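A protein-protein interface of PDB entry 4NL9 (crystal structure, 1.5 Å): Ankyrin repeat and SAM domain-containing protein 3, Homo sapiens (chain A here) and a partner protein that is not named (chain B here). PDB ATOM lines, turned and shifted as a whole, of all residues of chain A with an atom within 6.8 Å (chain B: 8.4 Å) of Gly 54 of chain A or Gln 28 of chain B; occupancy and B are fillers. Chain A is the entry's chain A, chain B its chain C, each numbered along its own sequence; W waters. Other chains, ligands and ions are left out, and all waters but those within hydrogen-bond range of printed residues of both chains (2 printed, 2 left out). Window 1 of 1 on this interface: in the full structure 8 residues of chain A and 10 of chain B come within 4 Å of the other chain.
Among the printed residues, pairs that only touch across the chains: Leu 52 of chain A with Glu 27 of chain B (3.7 Å), Leu 52 of chain A with Gln 28 of chain B (3.6 Å), Leu 52 of chain A with Glu 29 of chain B (3.4 Å), Phe 53 of chain A with Leu 38 of chain B (3.5 Å), Phe 53 of chain A with Leu 46 of chain B (3.7 Å), Gly 54 of chain A with Glu 29 of chain B (3.3 Å), Gly 54 of chain A with Val 30 of chain B (3.99 Å), Pro 55 of chain A with Gln 28 of chain B (3.6 Å), Pro 55 of chain A with Glu 29 of chain B (3.7 Å) and Lys 58 of chain A with Glu 33 of chain B (3.8 Å).
The backbone carbonyl oxygen of Phe 25 of chain B sits at hydrogen-bond distance from the backbone NH of Val 30 of chain B (3.0 Å). The side-chain carboxylate of Asp 31 of chain B sits at hydrogen-bond distance from the backbone NH of Ala 34 of chain B. The backbone carbonyl oxygen of Ala 34 of chain B sits at hydrogen-bond distance from the side-chain hydroxyl of Thr 37 of chain B (2.7 Å).
NZ of Lys 58 of chain A is in salt-bridge range of OD2 of Asp 31 of chain B, 2.9 Å away. The side-chain hydroxyl (OG1) of Thr 37 of chain B sits at hydrogen-bond distance from the guanidinium group (NH2) of Arg 57 of chain A. N of Gly 54 of chain A is in hydrogen-bond range of O of Gln 28 of chain B (2.9 Å). N of Phe 53 of chain A sits at hydrogen-bond distance from OE1 of Gln 28 of chain B (2.8 Å).
Water W1 lies within hydrogen-bond range of the backbone carbonyl oxygen (O) of Glu 29 of chain B (2.7 Å) and the side-chain amino group (NZ) of Lys 58 of chain A (2.9 Å). Water W2 lies within hydrogen-bond range of OE2 of Glu 45 of chain B (3.4 Å) and NZ of Lys 56 of chain A (3.4 Å).
Printed residues of chain B within 4 Å of Gly 54 of chain A: Gln 28, Glu 29 and Val 30. Pro 55 of chain A touches just these residues of chain B: Gln 28 (3.6 Å) and Glu 29 (3.7 Å). Printed residues of chain B within 4 Å of Arg 57 of chain A: Thr 37. Gln 28 of chain B touches just these residues of chain A: Leu 52 (3.6 Å), Phe 53 (2.8 Å), Gly 54 (2.9 Å) and Pro 55 (3.6 Å). Printed residues of chain A within 4 Å of Glu 29 of chain B: Leu 52 (3.4 Å), Gly 54 (3.3 Å) and Pro 55 (3.7 Å). Printed residues of chain A within 4 Å of Val 30 of chain B: Gly 54 (3.99 Å). Printed residues of chain A within 4 Å of Glu 33 of chain B: Lys 58. The nearest printed residue of chain B that does not touch Gly 54 of chain A is Ala 34 of chain B (4.2 Å). The nearest residue of chain A that does not touch Gln 28 of chain B is Thr 51 of chain A (4.3 Å). The nearest printed residue of chain A that does not touch Glu 29 of chain B is Lys 58 of chain A (5.3 Å).
Printed residues of chain B that touch a printed residue of chain A: Glu 27, Gln 28, Glu 29, Val 30, Asp 31, Glu 33, Thr 37, Leu 38 and Leu 46. Hydrophobic or aromatic side chains of chain B within 4 Å of the printed part of chain A: Val 30, Leu 38 and Leu 46. Hydrophobic or aromatic side chains of chain A that line the printed part of chain B: Leu 52, Phe 53 and Pro 55. Among the printed residues, Asp or Glu carboxylates within 4 Å of a Lys or Arg side-chain nitrogen of the other chain: Lys 58 of chain A with Asp 31 of chain B (2.9 Å).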
ATOM      1  N   CYS A  20     -18.362   6.240  26.552  1.00  0.00           N
ATOM      2  CA  CYS A  20     -19.006   5.738  25.348  1.00  0.00           C
ATOM      3  C   CYS A  20     -20.530   5.706  25.434  1.00  0.00           C
ATOM      4  O   CYS A  20     -21.181   4.922  24.737  1.00  0.00           O
ATOM      5  CB  CYS A  20     -18.471   4.346  25.015  1.00  0.00           C
ATOM      6  SG  CYS A  20     -16.793   4.367  24.304  1.00  0.00           S
ATOM      7  N   ILE A  50     -20.360   0.013  15.968  1.00  0.00           N
ATOM      8  CA  ILE A  50     -19.228   0.681  16.602  1.00  0.00           C
ATOM      9  C   ILE A  50     -18.094   0.649  15.587  1.00  0.00           C
ATOM     10  O   ILE A  50     -17.218  -0.212  15.643  1.00  0.00           O
ATOM     11  CB  ILE A  50     -18.795   0.017  17.938  1.00  0.00           C
ATOM     12  CG1 ILE A  50     -20.004  -0.364  18.805  1.00  0.00           C
ATOM     13  CG2 ILE A  50     -17.869   0.949  18.724  1.00  0.00           C
ATOM     14  CD1 ILE A  50     -20.994   0.772  19.060  1.00  0.00           C
ATOM     15  N   THR A  51     -18.145   1.576  14.632  1.00  0.00           N
ATOM     16  CA  THR A  51     -17.276   1.488  13.459  1.00  0.00           C
ATOM     17  C   THR A  51     -15.971   2.242  13.603  1.00  0.00           C
ATOM     18  O   THR A  51     -15.042   1.995  12.829  1.00  0.00           O
ATOM     19  CB  THR A  51     -17.982   1.977  12.174  1.00  0.00           C
ATOM     20  OG1 THR A  51     -18.153   3.401  12.213  1.00  0.00           O
ATOM     21  CG2 THR A  51     -19.334   1.305  12.013  1.00  0.00           C
ATOM     22  N   LEU A  52     -15.871   3.121  14.590  1.00  0.00           N
ATOM     23  CA  LEU A  52     -14.649   3.911  14.769  1.00  0.00           C
ATOM     24  C   LEU A  52     -13.637   3.227  15.677  1.00  0.00           C
ATOM     25  O   LEU A  52     -14.001   2.519  16.626  1.00  0.00           O
ATOM     26  CB  LEU A  52     -14.990   5.294  15.299  1.00  0.00           C
ATOM     27  CG  LEU A  52     -16.038   6.055  14.488  1.00  0.00           C
ATOM     28  CD1 LEU A  52     -16.332   7.394  15.135  1.00  0.00           C
ATOM     29  CD2 LEU A  52     -15.552   6.258  13.048  1.00  0.00           C
ATOM     30  N   PHE A  53     -12.351   3.422  15.390  1.00  0.00           N
ATOM     31  CA  PHE A  53     -11.327   2.660  16.081  1.00  0.00           C
ATOM     32  C   PHE A  53     -11.314   2.902  17.597  1.00  0.00           C
ATOM     33  O   PHE A  53     -11.197   1.959  18.393  1.00  0.00           O
ATOM     34  CB  PHE A  53      -9.941   2.978  15.507  1.00  0.00           C
ATOM     35  CG  PHE A  53      -8.887   2.001  15.932  1.00  0.00           C
ATOM     36  CD1 PHE A  53      -8.315   2.073  17.191  1.00  0.00           C
ATOM     37  CD2 PHE A  53      -8.506   0.982  15.086  1.00  0.00           C
ATOM     38  CE1 PHE A  53      -7.367   1.132  17.591  1.00  0.00           C
ATOM     39  CE2 PHE A  53      -7.556   0.052  15.479  1.00  0.00           C
ATOM     40  CZ  PHE A  53      -6.996   0.134  16.731  1.00  0.00           C
ATOM     41  N   GLY A  54     -11.398   4.167  17.993  1.00  0.00           N
ATOM     42  CA  GLY A  54     -11.263   4.542  19.387  1.00  0.00           C
ATOM     43  C   GLY A  54     -12.291   3.906  20.304  1.00  0.00           C
ATOM     44  O   GLY A  54     -11.924   3.192  21.234  1.00  0.00           O
ATOM     45  N   PRO A  55     -13.578   4.150  20.034  1.00  0.00           N
ATOM     46  CA  PRO A  55     -14.610   3.566  20.901  1.00  0.00           C
ATOM     47  C   PRO A  55     -14.578   2.044  20.890  1.00  0.00           C
ATOM     48  O   PRO A  55     -14.771   1.414  21.929  1.00  0.00           O
ATOM     49  CB  PRO A  55     -15.911   4.051  20.265  1.00  0.00           C
ATOM     50  CG  PRO A  55     -15.552   5.260  19.495  1.00  0.00           C
ATOM     51  CD  PRO A  55     -14.131   5.112  19.064  1.00  0.00           C
ATOM     52  N   LYS A  56     -14.332   1.456  19.727  1.00  0.00           N
ATOM     53  CA  LYS A  56     -14.309   0.002  19.639  1.00  0.00           C
ATOM     54  C   LYS A  56     -13.165  -0.552  20.485  1.00  0.00           C
ATOM     55  O   LYS A  56     -13.309  -1.592  21.135  1.00  0.00           O
ATOM     56  CB  LYS A  56     -14.236  -0.442  18.175  1.00  0.00           C
ATOM     57  CG  LYS A  56     -14.157  -1.936  17.947  1.00  0.00           C
ATOM     58  CD  LYS A  56     -14.646  -2.318  16.538  1.00  0.00           C
ATOM     59  CE  LYS A  56     -14.133  -1.377  15.465  1.00  0.00           C
ATOM     60  NZ  LYS A  56     -12.648  -1.511  15.331  1.00  0.00           N
ATOM     61  N   ARG A  57     -12.027   0.142  20.490  1.00  0.00           N
ATOM     62  CA  ARG A  57     -10.891  -0.298  21.297  1.00  0.00           C
ATOM     63  C   ARG A  57     -11.162  -0.139  22.798  1.00  0.00           C
ATOM     64  O   ARG A  57     -10.819  -1.015  23.600  1.00  0.00           O
ATOM     65  CB  ARG A  57      -9.619   0.456  20.880  1.00  0.00           C
ATOM     66  CG  ARG A  57      -8.399   0.228  21.782  1.00  0.00           C
ATOM     67  CD  ARG A  57      -8.000  -1.239  21.917  1.00  0.00           C
ATOM     68  NE  ARG A  57      -7.798  -1.903  20.634  1.00  0.00           N
ATOM     69  CZ  ARG A  57      -6.657  -1.905  19.948  1.00  0.00           C
ATOM     70  NH1 ARG A  57      -6.590  -2.567  18.801  1.00  0.00           N
ATOM     71  NH2 ARG A  57      -5.590  -1.250  20.399  1.00  0.00           N
ATOM     72  N   LYS A  58     -11.800   0.960  23.196  1.00  0.00           N
ATOM     73  CA  LYS A  58     -12.117   1.123  24.609  1.00  0.00           C
ATOM     74  C   LYS A  58     -13.095   0.049  25.056  1.00  0.00           C
ATOM     75  O   LYS A  58     -13.019  -0.438  26.183  1.00  0.00           O
ATOM     76  CB  LYS A  58     -12.651   2.518  24.893  1.00  0.00           C
ATOM     77  CG  LYS A  58     -11.567   3.574  24.713  1.00  0.00           C
ATOM     78  CD  LYS A  58     -11.953   4.903  25.312  1.00  0.00           C
ATOM     79  CE  LYS A  58     -13.088   5.532  24.531  1.00  0.00           C
ATOM     80  NZ  LYS A  58     -13.397   6.923  24.983  1.00  0.00           N
ATOM     81  N   MET A  59     -13.985  -0.346  24.149  1.00  0.00           N
ATOM     82  CA  MET A  59     -14.932  -1.411  24.468  1.00  0.00           C
ATOM     83  C   MET A  59     -14.280  -2.785  24.553  1.00  0.00           C
ATOM     84  O   MET A  59     -14.559  -3.540  25.476  1.00  0.00           O
ATOM     85  CB  MET A  59     -16.092  -1.434  23.481  1.00  0.00           C
ATOM     86  CG  MET A  59     -17.018  -0.244  23.625  1.00  0.00           C
ATOM     87  SD  MET A  59     -18.246  -0.248  22.303  1.00  0.00           S
ATOM     88  CE  MET A  59     -18.852   1.438  22.389  1.00  0.00           C
ATOM     89  N   TYR B  21      -1.041  13.493  10.668  1.00  0.00           N
ATOM     90  CA  TYR B  21      -1.907  12.363  10.980  1.00  0.00           C
ATOM     91  C   TYR B  21      -3.000  12.684  11.998  1.00  0.00           C
ATOM     92  O   TYR B  21      -3.867  11.858  12.261  1.00  0.00           O
ATOM     93  CB  TYR B  21      -1.080  11.176  11.488  1.00  0.00           C
ATOM     94  CG  TYR B  21      -0.067  10.656  10.498  1.00  0.00           C
ATOM     95  CD1 TYR B  21      -0.458  10.217   9.242  1.00  0.00           C
ATOM     96  CD2 TYR B  21       1.282  10.605  10.824  1.00  0.00           C
ATOM     97  CE1 TYR B  21       0.469   9.731   8.332  1.00  0.00           C
ATOM     98  CE2 TYR B  21       2.215  10.127   9.928  1.00  0.00           C
ATOM     99  CZ  TYR B  21       1.804   9.690   8.682  1.00  0.00           C
ATOM    100  OH  TYR B  21       2.749   9.209   7.793  1.00  0.00           O
ATOM    101  N   GLN B  22      -2.964  13.875  12.573  1.00  0.00           N
ATOM    102  CA  GLN B  22      -3.974  14.257  13.557  1.00  0.00           C
ATOM    103  C   GLN B  22      -5.423  14.012  13.086  1.00  0.00           C
ATOM    104  O   GLN B  22      -6.242  13.515  13.870  1.00  0.00           O
ATOM    105  CB  GLN B  22      -3.765  15.709  14.002  1.00  0.00           C
ATOM    106  CG  GLN B  22      -4.531  16.088  15.275  1.00  0.00           C
ATOM    107  CD  GLN B  22      -5.994  16.400  15.018  1.00  0.00           C
ATOM    108  OE1 GLN B  22      -6.363  16.860  13.935  1.00  0.00           O
ATOM    109  NE2 GLN B  22      -6.838  16.145  16.014  1.00  0.00           N
ATOM    110  N   PRO B  23      -5.747  14.331  11.813  1.00  0.00           N
ATOM    111  CA  PRO B  23      -7.138  14.115  11.396  1.00  0.00           C
ATOM    112  C   PRO B  23      -7.606  12.661  11.496  1.00  0.00           C
ATOM    113  O   PRO B  23      -8.799  12.419  11.721  1.00  0.00           O
ATOM    114  CB  PRO B  23      -7.138  14.583   9.937  1.00  0.00           C
ATOM    115  CG  PRO B  23      -6.055  15.624   9.886  1.00  0.00           C
ATOM    116  CD  PRO B  23      -4.989  15.081  10.784  1.00  0.00           C
ATOM    117  N   ILE B  24      -6.685  11.715  11.340  1.00  0.00           N
ATOM    118  CA  ILE B  24      -7.044  10.304  11.478  1.00  0.00           C
ATOM    119  C   ILE B  24      -7.500  10.012  12.896  1.00  0.00           C
ATOM    120  O   ILE B  24      -8.571   9.429  13.117  1.00  0.00           O
ATOM    121  CB  ILE B  24      -5.857   9.382  11.160  1.00  0.00           C
ATOM    122  CG1 ILE B  24      -5.479   9.485   9.682  1.00  0.00           C
ATOM    123  CG2 ILE B  24      -6.229   7.928  11.463  1.00  0.00           C
ATOM    124  CD1 ILE B  24      -4.212   8.709   9.328  1.00  0.00           C
ATOM    125  N   PHE B  25      -6.684  10.417  13.864  1.00  0.00           N
ATOM    126  CA  PHE B  25      -7.001  10.142  15.258  1.00  0.00           C
ATOM    127  C   PHE B  25      -8.270  10.850  15.695  1.00  0.00           C
ATOM    128  O   PHE B  25      -9.087  10.282  16.421  1.00  0.00           O
ATOM    129  CB  PHE B  25      -5.811  10.489  16.156  1.00  0.00           C
ATOM    130  CG  PHE B  25      -4.580   9.661  15.872  1.00  0.00           C
ATOM    131  CD1 PHE B  25      -4.498   8.347  16.303  1.00  0.00           C
ATOM    132  CD2 PHE B  25      -3.517  10.198  15.172  1.00  0.00           C
ATOM    133  CE1 PHE B  25      -3.376   7.575  16.047  1.00  0.00           C
ATOM    134  CE2 PHE B  25      -2.383   9.432  14.911  1.00  0.00           C
ATOM    135  CZ  PHE B  25      -2.313   8.121  15.343  1.00  0.00           C
ATOM    136  N   GLU B  26      -8.461  12.071  15.211  1.00  0.00           N
ATOM    137  CA  GLU B  26      -9.645  12.832  15.574  1.00  0.00           C
ATOM    138  C   GLU B  26     -10.914  12.172  15.040  1.00  0.00           C
ATOM    139  O   GLU B  26     -11.891  11.970  15.785  1.00  0.00           O
ATOM    140  CB  GLU B  26      -9.523  14.267  15.055  1.00  0.00           C
ATOM    141  CG  GLU B  26     -10.643  15.175  15.543  1.00  0.00           C
ATOM    142  CD  GLU B  26     -10.549  16.586  14.994  1.00  0.00           C
ATOM    143  OE1 GLU B  26      -9.444  16.997  14.576  1.00  0.00           O
ATOM    144  OE2 GLU B  26     -11.586  17.281  14.982  1.00  0.00           O
ATOM    145  N   GLU B  27     -10.912  11.825  13.758  1.00  0.00           N
ATOM    146  CA  GLU B  27     -12.119  11.255  13.165  1.00  0.00           C
ATOM    147  C   GLU B  27     -12.425   9.861  13.704  1.00  0.00           C
ATOM    148  O   GLU B  27     -13.590   9.461  13.785  1.00  0.00           O
ATOM    149  CB  GLU B  27     -12.016  11.231  11.640  1.00  0.00           C
ATOM    150  CG  GLU B  27     -13.345  10.985  10.946  1.00  0.00           C
ATOM    151  CD  GLU B  27     -13.260  11.328   9.483  1.00  0.00           C
ATOM    152  OE1 GLU B  27     -13.834  12.369   9.077  1.00  0.00           O
ATOM    153  OE2 GLU B  27     -12.586  10.582   8.755  1.00  0.00           O
ATOM    154  N   GLN B  28     -11.382   9.124  14.070  1.00  0.00           N
ATOM    155  CA  GLN B  28     -11.550   7.778  14.604  1.00  0.00           C
ATOM    156  C   GLN B  28     -11.774   7.792  16.113  1.00  0.00           C
ATOM    157  O   GLN B  28     -11.882   6.737  16.740  1.00  0.00           O
ATOM    158  CB  GLN B  28     -10.372   6.882  14.210  1.00  0.00           C
ATOM    159  CG  GLN B  28     -10.351   6.585  12.721  1.00  0.00           C
ATOM    160  CD  GLN B  28     -11.472   5.666  12.299  1.00  0.00           C
ATOM    161  OE1 GLN B  28     -11.681   4.603  12.897  1.00  0.00           O
ATOM    162  NE2 GLN B  28     -12.203   6.061  11.265  1.00  0.00           N
ATOM    163  N   GLU B  29     -11.863   8.996  16.675  1.00  0.00           N
ATOM    164  CA  GLU B  29     -12.173   9.185  18.091  1.00  0.00           C
ATOM    165  C   GLU B  29     -11.202   8.420  18.982  1.00  0.00           C
ATOM    166  O   GLU B  29     -11.585   7.795  19.973  1.00  0.00           O
ATOM    167  CB  GLU B  29     -13.643   8.856  18.387  1.00  0.00           C
ATOM    168  CG  GLU B  29     -14.598   9.849  17.716  1.00  0.00           C
ATOM    169  CD  GLU B  29     -16.070   9.531  17.925  1.00  0.00           C
ATOM    170  OE1 GLU B  29     -16.404   8.768  18.857  1.00  0.00           O
ATOM    171  OE2 GLU B  29     -16.893  10.048  17.140  1.00  0.00           O
ATOM    172  N   VAL B  30      -9.927   8.486  18.613  1.00  0.00           N
ATOM    173  CA  VAL B  30      -8.871   7.906  19.418  1.00  0.00           C
ATOM    174  C   VAL B  30      -8.421   8.897  20.488  1.00  0.00           C
ATOM    175  O   VAL B  30      -7.711   9.849  20.194  1.00  0.00           O
ATOM    176  CB  VAL B  30      -7.689   7.475  18.535  1.00  0.00           C
ATOM    177  CG1 VAL B  30      -6.575   6.904  19.386  1.00  0.00           C
ATOM    178  CG2 VAL B  30      -8.163   6.453  17.511  1.00  0.00           C
ATOM    179  N   ASP B  31      -8.876   8.684  21.721  1.00  0.00           N
ATOM    180  CA  ASP B  31      -8.380   9.456  22.858  1.00  0.00           C
ATOM    181  C   ASP B  31      -7.072   8.868  23.391  1.00  0.00           C
ATOM    182  O   ASP B  31      -6.561   7.887  22.843  1.00  0.00           O
ATOM    183  CB  ASP B  31      -9.439   9.564  23.968  1.00  0.00           C
ATOM    184  CG  ASP B  31      -9.872   8.208  24.523  1.00  0.00           C
ATOM    185  OD1 ASP B  31      -9.287   7.171  24.164  1.00  0.00           O
ATOM    186  OD2 ASP B  31     -10.818   8.184  25.344  1.00  0.00           O
ATOM    187  N   GLU B  33      -6.366   7.193  26.159  1.00  0.00           N
ATOM    188  CA  GLU B  33      -6.536   5.819  26.616  1.00  0.00           C
ATOM    189  C   GLU B  33      -6.390   4.833  25.460  1.00  0.00           C
ATOM    190  O   GLU B  33      -5.647   3.859  25.558  1.00  0.00           O
ATOM    191  CB  GLU B  33      -7.906   5.633  27.285  1.00  0.00           C
ATOM    192  CG  GLU B  33      -8.175   4.210  27.742  1.00  0.00           C
ATOM    193  CD  GLU B  33      -9.585   4.019  28.269  1.00  0.00           C
ATOM    194  OE1 GLU B  33     -10.196   5.012  28.717  1.00  0.00           O
ATOM    195  OE2 GLU B  33     -10.086   2.874  28.227  1.00  0.00           O
ATOM    196  N   ALA B  34      -7.095   5.095  24.365  1.00  0.00           N
ATOM    197  CA  ALA B  34      -7.004   4.234  23.198  1.00  0.00           C
ATOM    198  C   ALA B  34      -5.624   4.342  22.550  1.00  0.00           C
ATOM    199  O   ALA B  34      -5.055   3.338  22.129  1.00  0.00           O
ATOM    200  CB  ALA B  34      -8.100   4.576  22.199  1.00  0.00           C
ATOM    201  N   PHE B  35      -5.101   5.560  22.461  1.00  0.00           N
ATOM    202  CA  PHE B  35      -3.820   5.817  21.795  1.00  0.00           C
ATOM    203  C   PHE B  35      -2.698   4.986  22.405  1.00  0.00           C
ATOM    204  O   PHE B  35      -1.842   4.445  21.698  1.00  0.00           O
ATOM    205  CB  PHE B  35      -3.489   7.308  21.891  1.00  0.00           C
ATOM    206  CG  PHE B  35      -2.188   7.700  21.243  1.00  0.00           C
ATOM    207  CD1 PHE B  35      -2.085   7.790  19.861  1.00  0.00           C
ATOM    208  CD2 PHE B  35      -1.077   8.003  22.013  1.00  0.00           C
ATOM    209  CE1 PHE B  35      -0.883   8.159  19.257  1.00  0.00           C
ATOM    210  CE2 PHE B  35       0.118   8.391  21.424  1.00  0.00           C
ATOM    211  CZ  PHE B  35       0.216   8.468  20.041  1.00  0.00           C
ATOM    212  N   THR B  37      -2.771   2.172  23.615  1.00  0.00           N
ATOM    213  CA  THR B  37      -2.887   0.745  23.309  1.00  0.00           C
ATOM    214  C   THR B  37      -2.521   0.405  21.870  1.00  0.00           C
ATOM    215  O   THR B  37      -2.537  -0.766  21.493  1.00  0.00           O
ATOM    216  CB  THR B  37      -4.312   0.190  23.573  1.00  0.00           C
ATOM    217  OG1 THR B  37      -5.225   0.660  22.570  1.00  0.00           O
ATOM    218  CG2 THR B  37      -4.805   0.596  24.953  1.00  0.00           C
ATOM    219  N   LEU B  38      -2.173   1.411  21.074  1.00  0.00           N
ATOM    220  CA  LEU B  38      -1.970   1.191  19.646  1.00  0.00           C
ATOM    221  C   LEU B  38      -0.712   0.395  19.340  1.00  0.00           C
ATOM    222  O   LEU B  38       0.382   0.725  19.802  1.00  0.00           O
ATOM    223  CB  LEU B  38      -1.908   2.521  18.900  1.00  0.00           C
ATOM    224  CG  LEU B  38      -3.194   3.331  18.871  1.00  0.00           C
ATOM    225  CD1 LEU B  38      -2.913   4.694  18.230  1.00  0.00           C
ATOM    226  CD2 LEU B  38      -4.279   2.579  18.115  1.00  0.00           C
ATOM    227  N   GLU B  45      -3.680  -0.337  10.172  1.00  0.00           N
ATOM    228  CA  GLU B  45      -5.121  -0.376   9.947  1.00  0.00           C
ATOM    229  C   GLU B  45      -5.756   1.022   9.914  1.00  0.00           C
ATOM    230  O   GLU B  45      -6.689   1.274   9.148  1.00  0.00           O
ATOM    231  CB  GLU B  45      -5.788  -1.242  11.022  1.00  0.00           C
ATOM    232  CG  GLU B  45      -7.300  -1.364  10.890  1.00  0.00           C
ATOM    233  CD  GLU B  45      -7.907  -2.271  11.946  1.00  0.00           C
ATOM    234  OE1 GLU B  45      -7.229  -3.241  12.356  1.00  0.00           O
ATOM    235  OE2 GLU B  45      -9.055  -2.011  12.372  1.00  0.00           O
ATOM    236  N   LEU B  46      -5.245   1.923  10.750  1.00  0.00           N
ATOM    237  CA  LEU B  46      -5.721   3.306  10.785  1.00  0.00           C
ATOM    238  C   LEU B  46      -5.330   4.073   9.530  1.00  0.00           C
ATOM    239  O   LEU B  46      -5.927   5.101   9.218  1.00  0.00           O
ATOM    240  CB  LEU B  46      -5.179   4.043  12.015  1.00  0.00           C
ATOM    241  CG  LEU B  46      -5.865   3.732  13.346  1.00  0.00           C
ATOM    242  CD1 LEU B  46      -5.041   4.238  14.507  1.00  0.00           C
ATOM    243  CD2 LEU B  46      -7.243   4.355  13.381  1.00  0.00           C
ATOM    244  N   GLY B  47      -4.302   3.602   8.832  1.00  0.00           N
ATOM    245  CA  GLY B  47      -3.937   4.173   7.546  1.00  0.00           C
ATOM    246  C   GLY B  47      -2.537   4.751   7.472  1.00  0.00           C
ATOM    247  O   GLY B  47      -2.147   5.315   6.444  1.00  0.00           O
HETATM  248  O   HOH W   1     -13.212   7.668  22.186  1.00  0.00           O
HETATM  249  O   HOH W   2      -9.397  -2.476  15.730  1.00  0.00           O
